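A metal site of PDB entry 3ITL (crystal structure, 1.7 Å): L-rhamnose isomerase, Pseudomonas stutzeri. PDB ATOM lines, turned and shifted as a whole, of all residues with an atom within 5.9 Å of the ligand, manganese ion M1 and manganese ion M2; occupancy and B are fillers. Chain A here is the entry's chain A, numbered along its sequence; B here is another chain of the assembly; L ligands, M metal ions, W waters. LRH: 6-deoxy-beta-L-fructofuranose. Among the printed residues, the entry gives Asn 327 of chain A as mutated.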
ATOM      1  N   TRP A  57      -9.469 -16.674 -19.296  1.00  0.00           N
ATOM      2  CA  TRP A  57      -8.389 -15.819 -19.774  1.00  0.00           C
ATOM      3  C   TRP A  57      -8.251 -15.742 -21.292  1.00  0.00           C
ATOM      4  O   TRP A  57      -7.430 -14.981 -21.807  1.00  0.00           O
ATOM      5  CB  TRP A  57      -7.055 -16.280 -19.162  1.00  0.00           C
ATOM      6  CG  TRP A  57      -6.656 -17.677 -19.538  1.00  0.00           C
ATOM      7  CD1 TRP A  57      -5.843 -18.049 -20.570  1.00  0.00           C
ATOM      8  CD2 TRP A  57      -7.042 -18.885 -18.874  1.00  0.00           C
ATOM      9  NE1 TRP A  57      -5.716 -19.422 -20.598  1.00  0.00           N
ATOM     10  CE2 TRP A  57      -6.434 -19.954 -19.570  1.00  0.00           C
ATOM     11  CE3 TRP A  57      -7.848 -19.169 -17.769  1.00  0.00           C
ATOM     12  CZ2 TRP A  57      -6.615 -21.287 -19.187  1.00  0.00           C
ATOM     13  CZ3 TRP A  57      -8.026 -20.493 -17.385  1.00  0.00           C
ATOM     14  CH2 TRP A  57      -7.410 -21.541 -18.098  1.00  0.00           C
ATOM     15  N   HIS A 101      -8.757 -19.079 -13.549  1.00  0.00           N
ATOM     16  CA  HIS A 101      -7.331 -19.038 -13.269  1.00  0.00           C
ATOM     17  C   HIS A 101      -7.169 -18.102 -12.067  1.00  0.00           C
ATOM     18  O   HIS A 101      -7.666 -16.985 -12.068  1.00  0.00           O
ATOM     19  CB  HIS A 101      -6.568 -18.488 -14.485  1.00  0.00           C
ATOM     20  CG  HIS A 101      -5.255 -19.166 -14.725  1.00  0.00           C
ATOM     21  ND1 HIS A 101      -4.236 -19.163 -13.804  1.00  0.00           N
ATOM     22  CD2 HIS A 101      -4.819 -19.900 -15.778  1.00  0.00           C
ATOM     23  CE1 HIS A 101      -3.213 -19.865 -14.275  1.00  0.00           C
ATOM     24  NE2 HIS A 101      -3.541 -20.322 -15.475  1.00  0.00           N
ATOM     25  N   TRP A 104      -5.812 -14.399 -11.185  1.00  0.00           N
ATOM     26  CA  TRP A 104      -6.458 -13.524 -12.155  1.00  0.00           C
ATOM     27  C   TRP A 104      -7.949 -13.363 -11.900  1.00  0.00           C
ATOM     28  O   TRP A 104      -8.468 -12.244 -11.941  1.00  0.00           O
ATOM     29  CB  TRP A 104      -6.280 -14.040 -13.591  1.00  0.00           C
ATOM     30  CG  TRP A 104      -4.862 -14.129 -14.041  1.00  0.00           C
ATOM     31  CD1 TRP A 104      -3.786 -13.451 -13.533  1.00  0.00           C
ATOM     32  CD2 TRP A 104      -4.370 -14.911 -15.139  1.00  0.00           C
ATOM     33  NE1 TRP A 104      -2.648 -13.769 -14.238  1.00  0.00           N
ATOM     34  CE2 TRP A 104      -2.981 -14.659 -15.227  1.00  0.00           C
ATOM     35  CE3 TRP A 104      -4.968 -15.800 -16.044  1.00  0.00           C
ATOM     36  CZ2 TRP A 104      -2.170 -15.274 -16.197  1.00  0.00           C
ATOM     37  CZ3 TRP A 104      -4.163 -16.403 -17.002  1.00  0.00           C
ATOM     38  CH2 TRP A 104      -2.780 -16.140 -17.079  1.00  0.00           C
ATOM     39  N   ASN A 127      -7.348 -23.521 -12.126  1.00  0.00           N
ATOM     40  CA  ASN A 127      -5.969 -23.421 -12.595  1.00  0.00           C
ATOM     41  C   ASN A 127      -5.206 -22.550 -11.607  1.00  0.00           C
ATOM     42  O   ASN A 127      -5.607 -21.417 -11.343  1.00  0.00           O
ATOM     43  CB  ASN A 127      -5.918 -22.772 -13.977  1.00  0.00           C
ATOM     44  CG  ASN A 127      -6.524 -23.647 -15.052  1.00  0.00           C
ATOM     45  OD1 ASN A 127      -5.854 -24.493 -15.649  1.00  0.00           O
ATOM     46  ND2 ASN A 127      -7.817 -23.472 -15.304  1.00  0.00           N
ATOM     47  N   SER A 128      -4.110 -23.076 -11.059  1.00  0.00           N
ATOM     48  CA  SER A 128      -3.292 -22.314 -10.124  1.00  0.00           C
ATOM     49  C   SER A 128      -2.243 -21.528 -10.903  1.00  0.00           C
ATOM     50  O   SER A 128      -1.935 -21.851 -12.041  1.00  0.00           O
ATOM     51  CB  SER A 128      -2.607 -23.260  -9.131  1.00  0.00           C
ATOM     52  OG  SER A 128      -1.855 -24.256  -9.805  1.00  0.00           O
ATOM     53  N   PHE A 131       3.560 -19.098 -11.596  1.00  0.00           N
ATOM     54  CA  PHE A 131       4.536 -18.818 -12.657  1.00  0.00           C
ATOM     55  C   PHE A 131       4.671 -17.300 -12.838  1.00  0.00           C
ATOM     56  O   PHE A 131       5.306 -16.824 -13.784  1.00  0.00           O
ATOM     57  CB  PHE A 131       4.115 -19.495 -13.966  1.00  0.00           C
ATOM     58  CG  PHE A 131       2.706 -19.190 -14.407  1.00  0.00           C
ATOM     59  CD1 PHE A 131       2.404 -17.972 -15.016  1.00  0.00           C
ATOM     60  CD2 PHE A 131       1.696 -20.128 -14.239  1.00  0.00           C
ATOM     61  CE1 PHE A 131       1.111 -17.701 -15.438  1.00  0.00           C
ATOM     62  CE2 PHE A 131       0.390 -19.864 -14.652  1.00  0.00           C
ATOM     63  CZ  PHE A 131       0.101 -18.640 -15.260  1.00  0.00           C
ATOM     64  N   THR A 177      -5.795 -28.023 -12.005  1.00  0.00           N
ATOM     65  CA  THR A 177      -4.749 -28.226 -13.011  1.00  0.00           C
ATOM     66  C   THR A 177      -3.529 -27.446 -12.547  1.00  0.00           C
ATOM     67  O   THR A 177      -3.623 -26.261 -12.229  1.00  0.00           O
ATOM     68  CB  THR A 177      -5.157 -27.698 -14.389  1.00  0.00           C
ATOM     69  OG1 THR A 177      -6.259 -28.473 -14.899  1.00  0.00           O
ATOM     70  CG2 THR A 177      -3.976 -27.793 -15.369  1.00  0.00           C
ATOM     71  N   TRP A 179       0.101 -26.218 -13.706  1.00  0.00           N
ATOM     72  CA  TRP A 179       1.122 -25.994 -14.713  1.00  0.00           C
ATOM     73  C   TRP A 179       2.041 -24.936 -14.123  1.00  0.00           C
ATOM     74  O   TRP A 179       1.580 -23.890 -13.678  1.00  0.00           O
ATOM     75  CB  TRP A 179       0.565 -25.441 -16.020  1.00  0.00           C
ATOM     76  CG  TRP A 179       1.696 -25.064 -16.946  1.00  0.00           C
ATOM     77  CD1 TRP A 179       2.540 -25.925 -17.591  1.00  0.00           C
ATOM     78  CD2 TRP A 179       2.194 -23.744 -17.202  1.00  0.00           C
ATOM     79  NE1 TRP A 179       3.543 -25.215 -18.229  1.00  0.00           N
ATOM     80  CE2 TRP A 179       3.351 -23.885 -18.007  1.00  0.00           C
ATOM     81  CE3 TRP A 179       1.776 -22.458 -16.828  1.00  0.00           C
ATOM     82  CZ2 TRP A 179       4.087 -22.779 -18.453  1.00  0.00           C
ATOM     83  CZ3 TRP A 179       2.517 -21.366 -17.266  1.00  0.00           C
ATOM     84  CH2 TRP A 179       3.658 -21.523 -18.063  1.00  0.00           C
ATOM     85  N   GLU A 219       0.474 -30.785 -15.665  1.00  0.00           N
ATOM     86  CA  GLU A 219       0.631 -30.542 -17.104  1.00  0.00           C
ATOM     87  C   GLU A 219       2.091 -30.369 -17.542  1.00  0.00           C
ATOM     88  O   GLU A 219       2.794 -29.488 -17.048  1.00  0.00           O
ATOM     89  CB  GLU A 219      -0.175 -29.287 -17.478  1.00  0.00           C
ATOM     90  CG  GLU A 219      -0.002 -28.825 -18.921  1.00  0.00           C
ATOM     91  CD  GLU A 219      -0.818 -27.575 -19.216  1.00  0.00           C
ATOM     92  OE1 GLU A 219      -1.315 -26.945 -18.257  1.00  0.00           O
ATOM     93  OE2 GLU A 219      -0.961 -27.233 -20.408  1.00  0.00           O
ATOM     94  N   LYS A 221       5.259 -29.569 -20.252  1.00  0.00           N
ATOM     95  CA  LYS A 221       5.559 -28.603 -21.300  1.00  0.00           C
ATOM     96  C   LYS A 221       7.068 -28.685 -21.555  1.00  0.00           C
ATOM     97  O   LYS A 221       7.856 -28.587 -20.629  1.00  0.00           O
ATOM     98  CB  LYS A 221       5.176 -27.195 -20.881  1.00  0.00           C
ATOM     99  CG  LYS A 221       5.246 -26.186 -22.020  1.00  0.00           C
ATOM    100  CD  LYS A 221       4.728 -24.825 -21.610  1.00  0.00           C
ATOM    101  CE  LYS A 221       4.775 -23.846 -22.782  1.00  0.00           C
ATOM    102  NZ  LYS A 221       4.426 -22.462 -22.366  1.00  0.00           N
ATOM    103  N   GLU A 224       9.508 -23.016 -22.229  1.00  0.00           N
ATOM    104  CA  GLU A 224       8.794 -21.739 -22.106  1.00  0.00           C
ATOM    105  C   GLU A 224       7.904 -21.763 -20.861  1.00  0.00           C
ATOM    106  O   GLU A 224       6.897 -22.481 -20.828  1.00  0.00           O
ATOM    107  CB  GLU A 224       7.933 -21.407 -23.336  1.00  0.00           C
ATOM    108  CG  GLU A 224       7.318 -20.006 -23.206  1.00  0.00           C
ATOM    109  CD  GLU A 224       6.192 -19.717 -24.176  1.00  0.00           C
ATOM    110  OE1 GLU A 224       5.395 -20.632 -24.464  1.00  0.00           O
ATOM    111  OE2 GLU A 224       6.078 -18.546 -24.614  1.00  0.00           O
ATOM    112  N   LEU A 252      -2.387 -33.992 -17.794  1.00  0.00           N
ATOM    113  CA  LEU A 252      -3.095 -33.140 -18.738  1.00  0.00           C
ATOM    114  C   LEU A 252      -2.201 -32.960 -19.954  1.00  0.00           C
ATOM    115  O   LEU A 252      -1.025 -32.604 -19.824  1.00  0.00           O
ATOM    116  CB  LEU A 252      -3.431 -31.787 -18.113  1.00  0.00           C
ATOM    117  CG  LEU A 252      -4.362 -30.938 -18.982  1.00  0.00           C
ATOM    118  CD1 LEU A 252      -5.531 -30.420 -18.153  1.00  0.00           C
ATOM    119  CD2 LEU A 252      -3.577 -29.805 -19.615  1.00  0.00           C
ATOM    120  N   ASP A 254      -1.495 -30.908 -23.301  1.00  0.00           N
ATOM    121  CA  ASP A 254      -1.740 -29.672 -24.048  1.00  0.00           C
ATOM    122  C   ASP A 254      -1.067 -29.886 -25.406  1.00  0.00           C
ATOM    123  O   ASP A 254       0.145 -30.063 -25.489  1.00  0.00           O
ATOM    124  CB  ASP A 254      -1.130 -28.478 -23.298  1.00  0.00           C
ATOM    125  CG  ASP A 254      -1.488 -27.151 -23.926  1.00  0.00           C
ATOM    126  OD1 ASP A 254      -1.899 -26.214 -23.191  1.00  0.00           O
ATOM    127  OD2 ASP A 254      -1.358 -27.022 -25.156  1.00  0.00           O
ATOM    128  N   HIS A 257       2.440 -28.336 -26.389  1.00  0.00           N
ATOM    129  CA  HIS A 257       3.560 -28.468 -25.461  1.00  0.00           C
ATOM    130  C   HIS A 257       4.564 -29.581 -25.770  1.00  0.00           C
ATOM    131  O   HIS A 257       5.302 -29.997 -24.875  1.00  0.00           O
ATOM    132  CB  HIS A 257       3.043 -28.673 -24.037  1.00  0.00           C
ATOM    133  CG  HIS A 257       2.324 -27.493 -23.472  1.00  0.00           C
ATOM    134  ND1 HIS A 257       1.999 -27.404 -22.130  1.00  0.00           N
ATOM    135  CD2 HIS A 257       1.877 -26.355 -24.044  1.00  0.00           C
ATOM    136  CE1 HIS A 257       1.394 -26.245 -21.907  1.00  0.00           C
ATOM    137  NE2 HIS A 257       1.313 -25.588 -23.050  1.00  0.00           N
ATOM    138  N   HIS A 281      -5.875 -29.845 -23.220  1.00  0.00           N
ATOM    139  CA  HIS A 281      -5.853 -28.401 -23.422  1.00  0.00           C
ATOM    140  C   HIS A 281      -5.757 -28.352 -24.935  1.00  0.00           C
ATOM    141  O   HIS A 281      -4.744 -28.725 -25.519  1.00  0.00           O
ATOM    142  CB  HIS A 281      -4.640 -27.737 -22.781  1.00  0.00           C
ATOM    143  CG  HIS A 281      -4.901 -27.182 -21.412  1.00  0.00           C
ATOM    144  ND1 HIS A 281      -4.048 -26.308 -20.785  1.00  0.00           N
ATOM    145  CD2 HIS A 281      -5.931 -27.393 -20.565  1.00  0.00           C
ATOM    146  CE1 HIS A 281      -4.541 -25.999 -19.592  1.00  0.00           C
ATOM    147  NE2 HIS A 281      -5.678 -26.643 -19.434  1.00  0.00           N
ATOM    148  N   ASN A 283      -5.800 -26.550 -28.702  1.00  0.00           N
ATOM    149  CA  ASN A 283      -5.313 -25.383 -29.419  1.00  0.00           C
ATOM    150  C   ASN A 283      -4.563 -25.947 -30.616  1.00  0.00           C
ATOM    151  O   ASN A 283      -4.488 -27.165 -30.788  1.00  0.00           O
ATOM    152  CB  ASN A 283      -4.366 -24.556 -28.533  1.00  0.00           C
ATOM    153  CG  ASN A 283      -3.285 -25.392 -27.861  1.00  0.00           C
ATOM    154  OD1 ASN A 283      -2.476 -26.056 -28.524  1.00  0.00           O
ATOM    155  ND2 ASN A 283      -3.270 -25.363 -26.527  1.00  0.00           N
ATOM    156  N   ASP A 289       4.509 -23.367 -28.594  1.00  0.00           N
ATOM    157  CA  ASP A 289       3.226 -23.359 -27.899  1.00  0.00           C
ATOM    158  C   ASP A 289       2.512 -22.109 -28.413  1.00  0.00           C
ATOM    159  O   ASP A 289       2.305 -21.140 -27.669  1.00  0.00           O
ATOM    160  CB  ASP A 289       3.451 -23.290 -26.384  1.00  0.00           C
ATOM    161  CG  ASP A 289       2.159 -23.430 -25.596  1.00  0.00           C
ATOM    162  OD1 ASP A 289       1.211 -24.046 -26.114  1.00  0.00           O
ATOM    163  OD2 ASP A 289       2.096 -22.931 -24.441  1.00  0.00           O
ATOM    164  N   ASP A 291      -0.585 -21.537 -29.286  1.00  0.00           N
ATOM    165  CA  ASP A 291      -1.910 -21.257 -28.751  1.00  0.00           C
ATOM    166  C   ASP A 291      -2.917 -20.697 -29.746  1.00  0.00           C
ATOM    167  O   ASP A 291      -3.757 -19.863 -29.406  1.00  0.00           O
ATOM    168  CB  ASP A 291      -1.786 -20.306 -27.558  1.00  0.00           C
ATOM    169  CG  ASP A 291      -1.198 -20.977 -26.334  1.00  0.00           C
ATOM    170  OD1 ASP A 291      -1.428 -22.197 -26.201  1.00  0.00           O
ATOM    171  OD2 ASP A 291      -0.527 -20.319 -25.515  1.00  0.00           O
ATOM    172  N   ASN A 327      -7.450 -24.057 -24.459  1.00  0.00           N
ATOM    173  CA  ASN A 327      -6.436 -23.208 -23.851  1.00  0.00           C
ATOM    174  C   ASN A 327      -5.752 -22.528 -25.024  1.00  0.00           C
ATOM    175  O   ASN A 327      -4.849 -23.083 -25.632  1.00  0.00           O
ATOM    176  CB  ASN A 327      -5.420 -24.027 -23.047  1.00  0.00           C
ATOM    177  CG  ASN A 327      -4.466 -23.144 -22.276  1.00  0.00           C
ATOM    178  OD1 ASN A 327      -4.885 -22.321 -21.464  1.00  0.00           O
ATOM    179  ND2 ASN A 327      -3.165 -23.301 -22.525  1.00  0.00           N
ATOM    180  N   ARG B  65       6.173 -14.102 -22.034  1.00  0.00           N
ATOM    181  CA  ARG B  65       4.786 -13.642 -22.063  1.00  0.00           C
ATOM    182  C   ARG B  65       4.050 -14.007 -20.774  1.00  0.00           C
ATOM    183  O   ARG B  65       2.968 -13.483 -20.506  1.00  0.00           O
ATOM    184  CB  ARG B  65       4.049 -14.228 -23.268  1.00  0.00           C
ATOM    185  CG  ARG B  65       4.053 -15.732 -23.344  1.00  0.00           C
ATOM    186  CD  ARG B  65       3.113 -16.236 -24.433  1.00  0.00           C
ATOM    187  NE  ARG B  65       3.266 -17.675 -24.609  1.00  0.00           N
ATOM    188  CZ  ARG B  65       2.296 -18.506 -24.972  1.00  0.00           C
ATOM    189  NH1 ARG B  65       1.070 -18.058 -25.210  1.00  0.00           N
ATOM    190  NH2 ARG B  65       2.556 -19.800 -25.088  1.00  0.00           N
ATOM    191  N   PHE B  66       4.636 -14.892 -19.978  1.00  0.00           N
ATOM    192  CA  PHE B  66       4.025 -15.319 -18.733  1.00  0.00           C
ATOM    193  C   PHE B  66       4.398 -14.449 -17.534  1.00  0.00           C
ATOM    194  O   PHE B  66       3.584 -14.275 -16.627  1.00  0.00           O
ATOM    195  CB  PHE B  66       4.380 -16.785 -18.434  1.00  0.00           C
ATOM    196  CG  PHE B  66       3.775 -17.748 -19.408  1.00  0.00           C
ATOM    197  CD1 PHE B  66       2.410 -18.049 -19.345  1.00  0.00           C
ATOM    198  CD2 PHE B  66       4.539 -18.284 -20.440  1.00  0.00           C
ATOM    199  CE1 PHE B  66       1.826 -18.873 -20.293  1.00  0.00           C
ATOM    200  CE2 PHE B  66       3.964 -19.111 -21.398  1.00  0.00           C
ATOM    201  CZ  PHE B  66       2.599 -19.412 -21.325  1.00  0.00           C
HETATM  202  C1  LRH L   1       1.088 -23.062 -20.139  1.00  0.00           C
HETATM  203  C2  LRH L   1      -0.417 -23.065 -20.246  1.00  0.00           C
HETATM  204  C3  LRH L   1      -1.156 -23.523 -18.978  1.00  0.00           C
HETATM  205  C4  LRH L   1      -2.036 -22.338 -18.577  1.00  0.00           C
HETATM  206  C5  LRH L   1      -1.481 -21.154 -19.371  1.00  0.00           C
HETATM  207  C6  LRH L   1      -2.552 -20.213 -19.880  1.00  0.00           C
HETATM  208  O1  LRH L   1       1.672 -22.680 -21.379  1.00  0.00           O
HETATM  209  O2  LRH L   1      -0.808 -23.876 -21.348  1.00  0.00           O
HETATM  210  O3  LRH L   1      -1.984 -24.640 -19.270  1.00  0.00           O
HETATM  211  O4  LRH L   1      -1.917 -22.086 -17.185  1.00  0.00           O
HETATM  212  O5  LRH L   1      -0.823 -21.713 -20.509  1.00  0.00           O
HETATM  213 MN    MN M   1      -2.010 -25.632 -21.191  1.00  0.00          MN
HETATM  214 MN    MN M   2       0.522 -23.579 -23.145  1.00  0.00          MN
HETATM  215  O   HOH W   1      -1.210 -23.798 -24.360  1.00  0.00           O
HETATM  216  O   HOH W   2      -2.987 -24.212 -15.850  1.00  0.00           O
HETATM  217  O   HOH W   3      -0.041 -21.502 -23.175  1.00  0.00           O
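O1 of the ligand lies close to NZ of Lys 221, at 2.9 Å.
O4 of the ligand sits at hydrogen-bond distance from NE2 of His 101, at 2.9 Å.
O5 of the ligand sits at hydrogen-bond distance from ND2 of Asn 327, 3.5 Å away.
The side-chain carboxylate (OD2) of Asp 254 is in hydrogen-bond range of the side-chain amide nitrogen (ND2) of Asn 283.
The side-chain carboxylate (OD2) of Asp 289 lies close to the side-chain amino group (NZ) of Lys 221, 3.2 Å away.
The side-chain amide nitrogen of Asn 327 lies close to the side-chain carboxylate of Asp 254.
OE2 of Glu 219 lies close to ND1 of His 257 (3.4 Å).
The guanidinium group of Arg 65 of chain B lies within hydrogen-bond range of the backbone carbonyl oxygen of Asp 289 (2.9 Å).
The indole nitrogen of Trp 57 sits close to the side-chain amide oxygen of Asn 327 (3.1 Å).
The side-chain carboxylate of Asp 291 is in salt-bridge range of the guanidinium group of Arg 65 of chain B.
The backbone carbonyl oxygen of Asn 327 sits at hydrogen-bond distance from the side-chain amide nitrogen of Asn 283 (2.9 Å).
Residues that only touch the ligand: Trp 179 (3.2 Å), Trp 57 (3.3 Å) and Phe 66 of chain B (3.4 Å).
Hydrophobic or aromatic side chains within 4 Å of the ligand: Trp 57, His 101, Trp 179, His 257, His 281 and Phe 66 of chain B.
Of the 21 residues printed, 11 come within 4 Å of the ligand.
Along chain A the residues within 4 Å of the ligand span positions 57 to 327.
The nearest printed residue that does not touch the ligand is Phe 131 (4.1 Å).
Of the 21 residues printed, 5 come within 4 Å of manganese ion M1.
Asp 291 touches manganese ion M2.
Manganese ion M1 is bound by OE2 of Glu 219, 2.1 Å away.
The side-chain carboxylate (OD1) of Asp 254 is bound to manganese ion M1 (2.1 Å).
O2 of the ligand binds manganese ion M1.
O3 of the ligand binds manganese ion M1, at 2.2 Å.
A ring nitrogen (ND1) of His 281 binds manganese ion M1 (2.2 Å).
Manganese ion M1 has five donor atoms within binding distance.
Slightly farther from manganese ion M1 lies ND2 of Asn 327 (2.9 Å).
Manganese ion M2 is bound by water W1, at 2.1 Å.
OD2 of Asp 289 is bound to manganese ion M2, at 2.1 Å.
Water W3 binds manganese ion M2, at 2.2 Å.
A ring nitrogen (NE2) of His 257 is bound to manganese ion M2, 2.2 Å away.
O2 of the ligand binds manganese ion M2, at 2.3 Å.
Manganese ion M2 is bound by an oxygen (O1) of the ligand.
Water W3 bridges OD2 of Asp 291 (2.7 Å) and O5 of the ligand (2.8 Å).
Water W2 bridges an oxygen (O4) of the ligand (2.7 Å) and the side-chain amide oxygen (OD1) of Asn 127 (2.9 Å).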
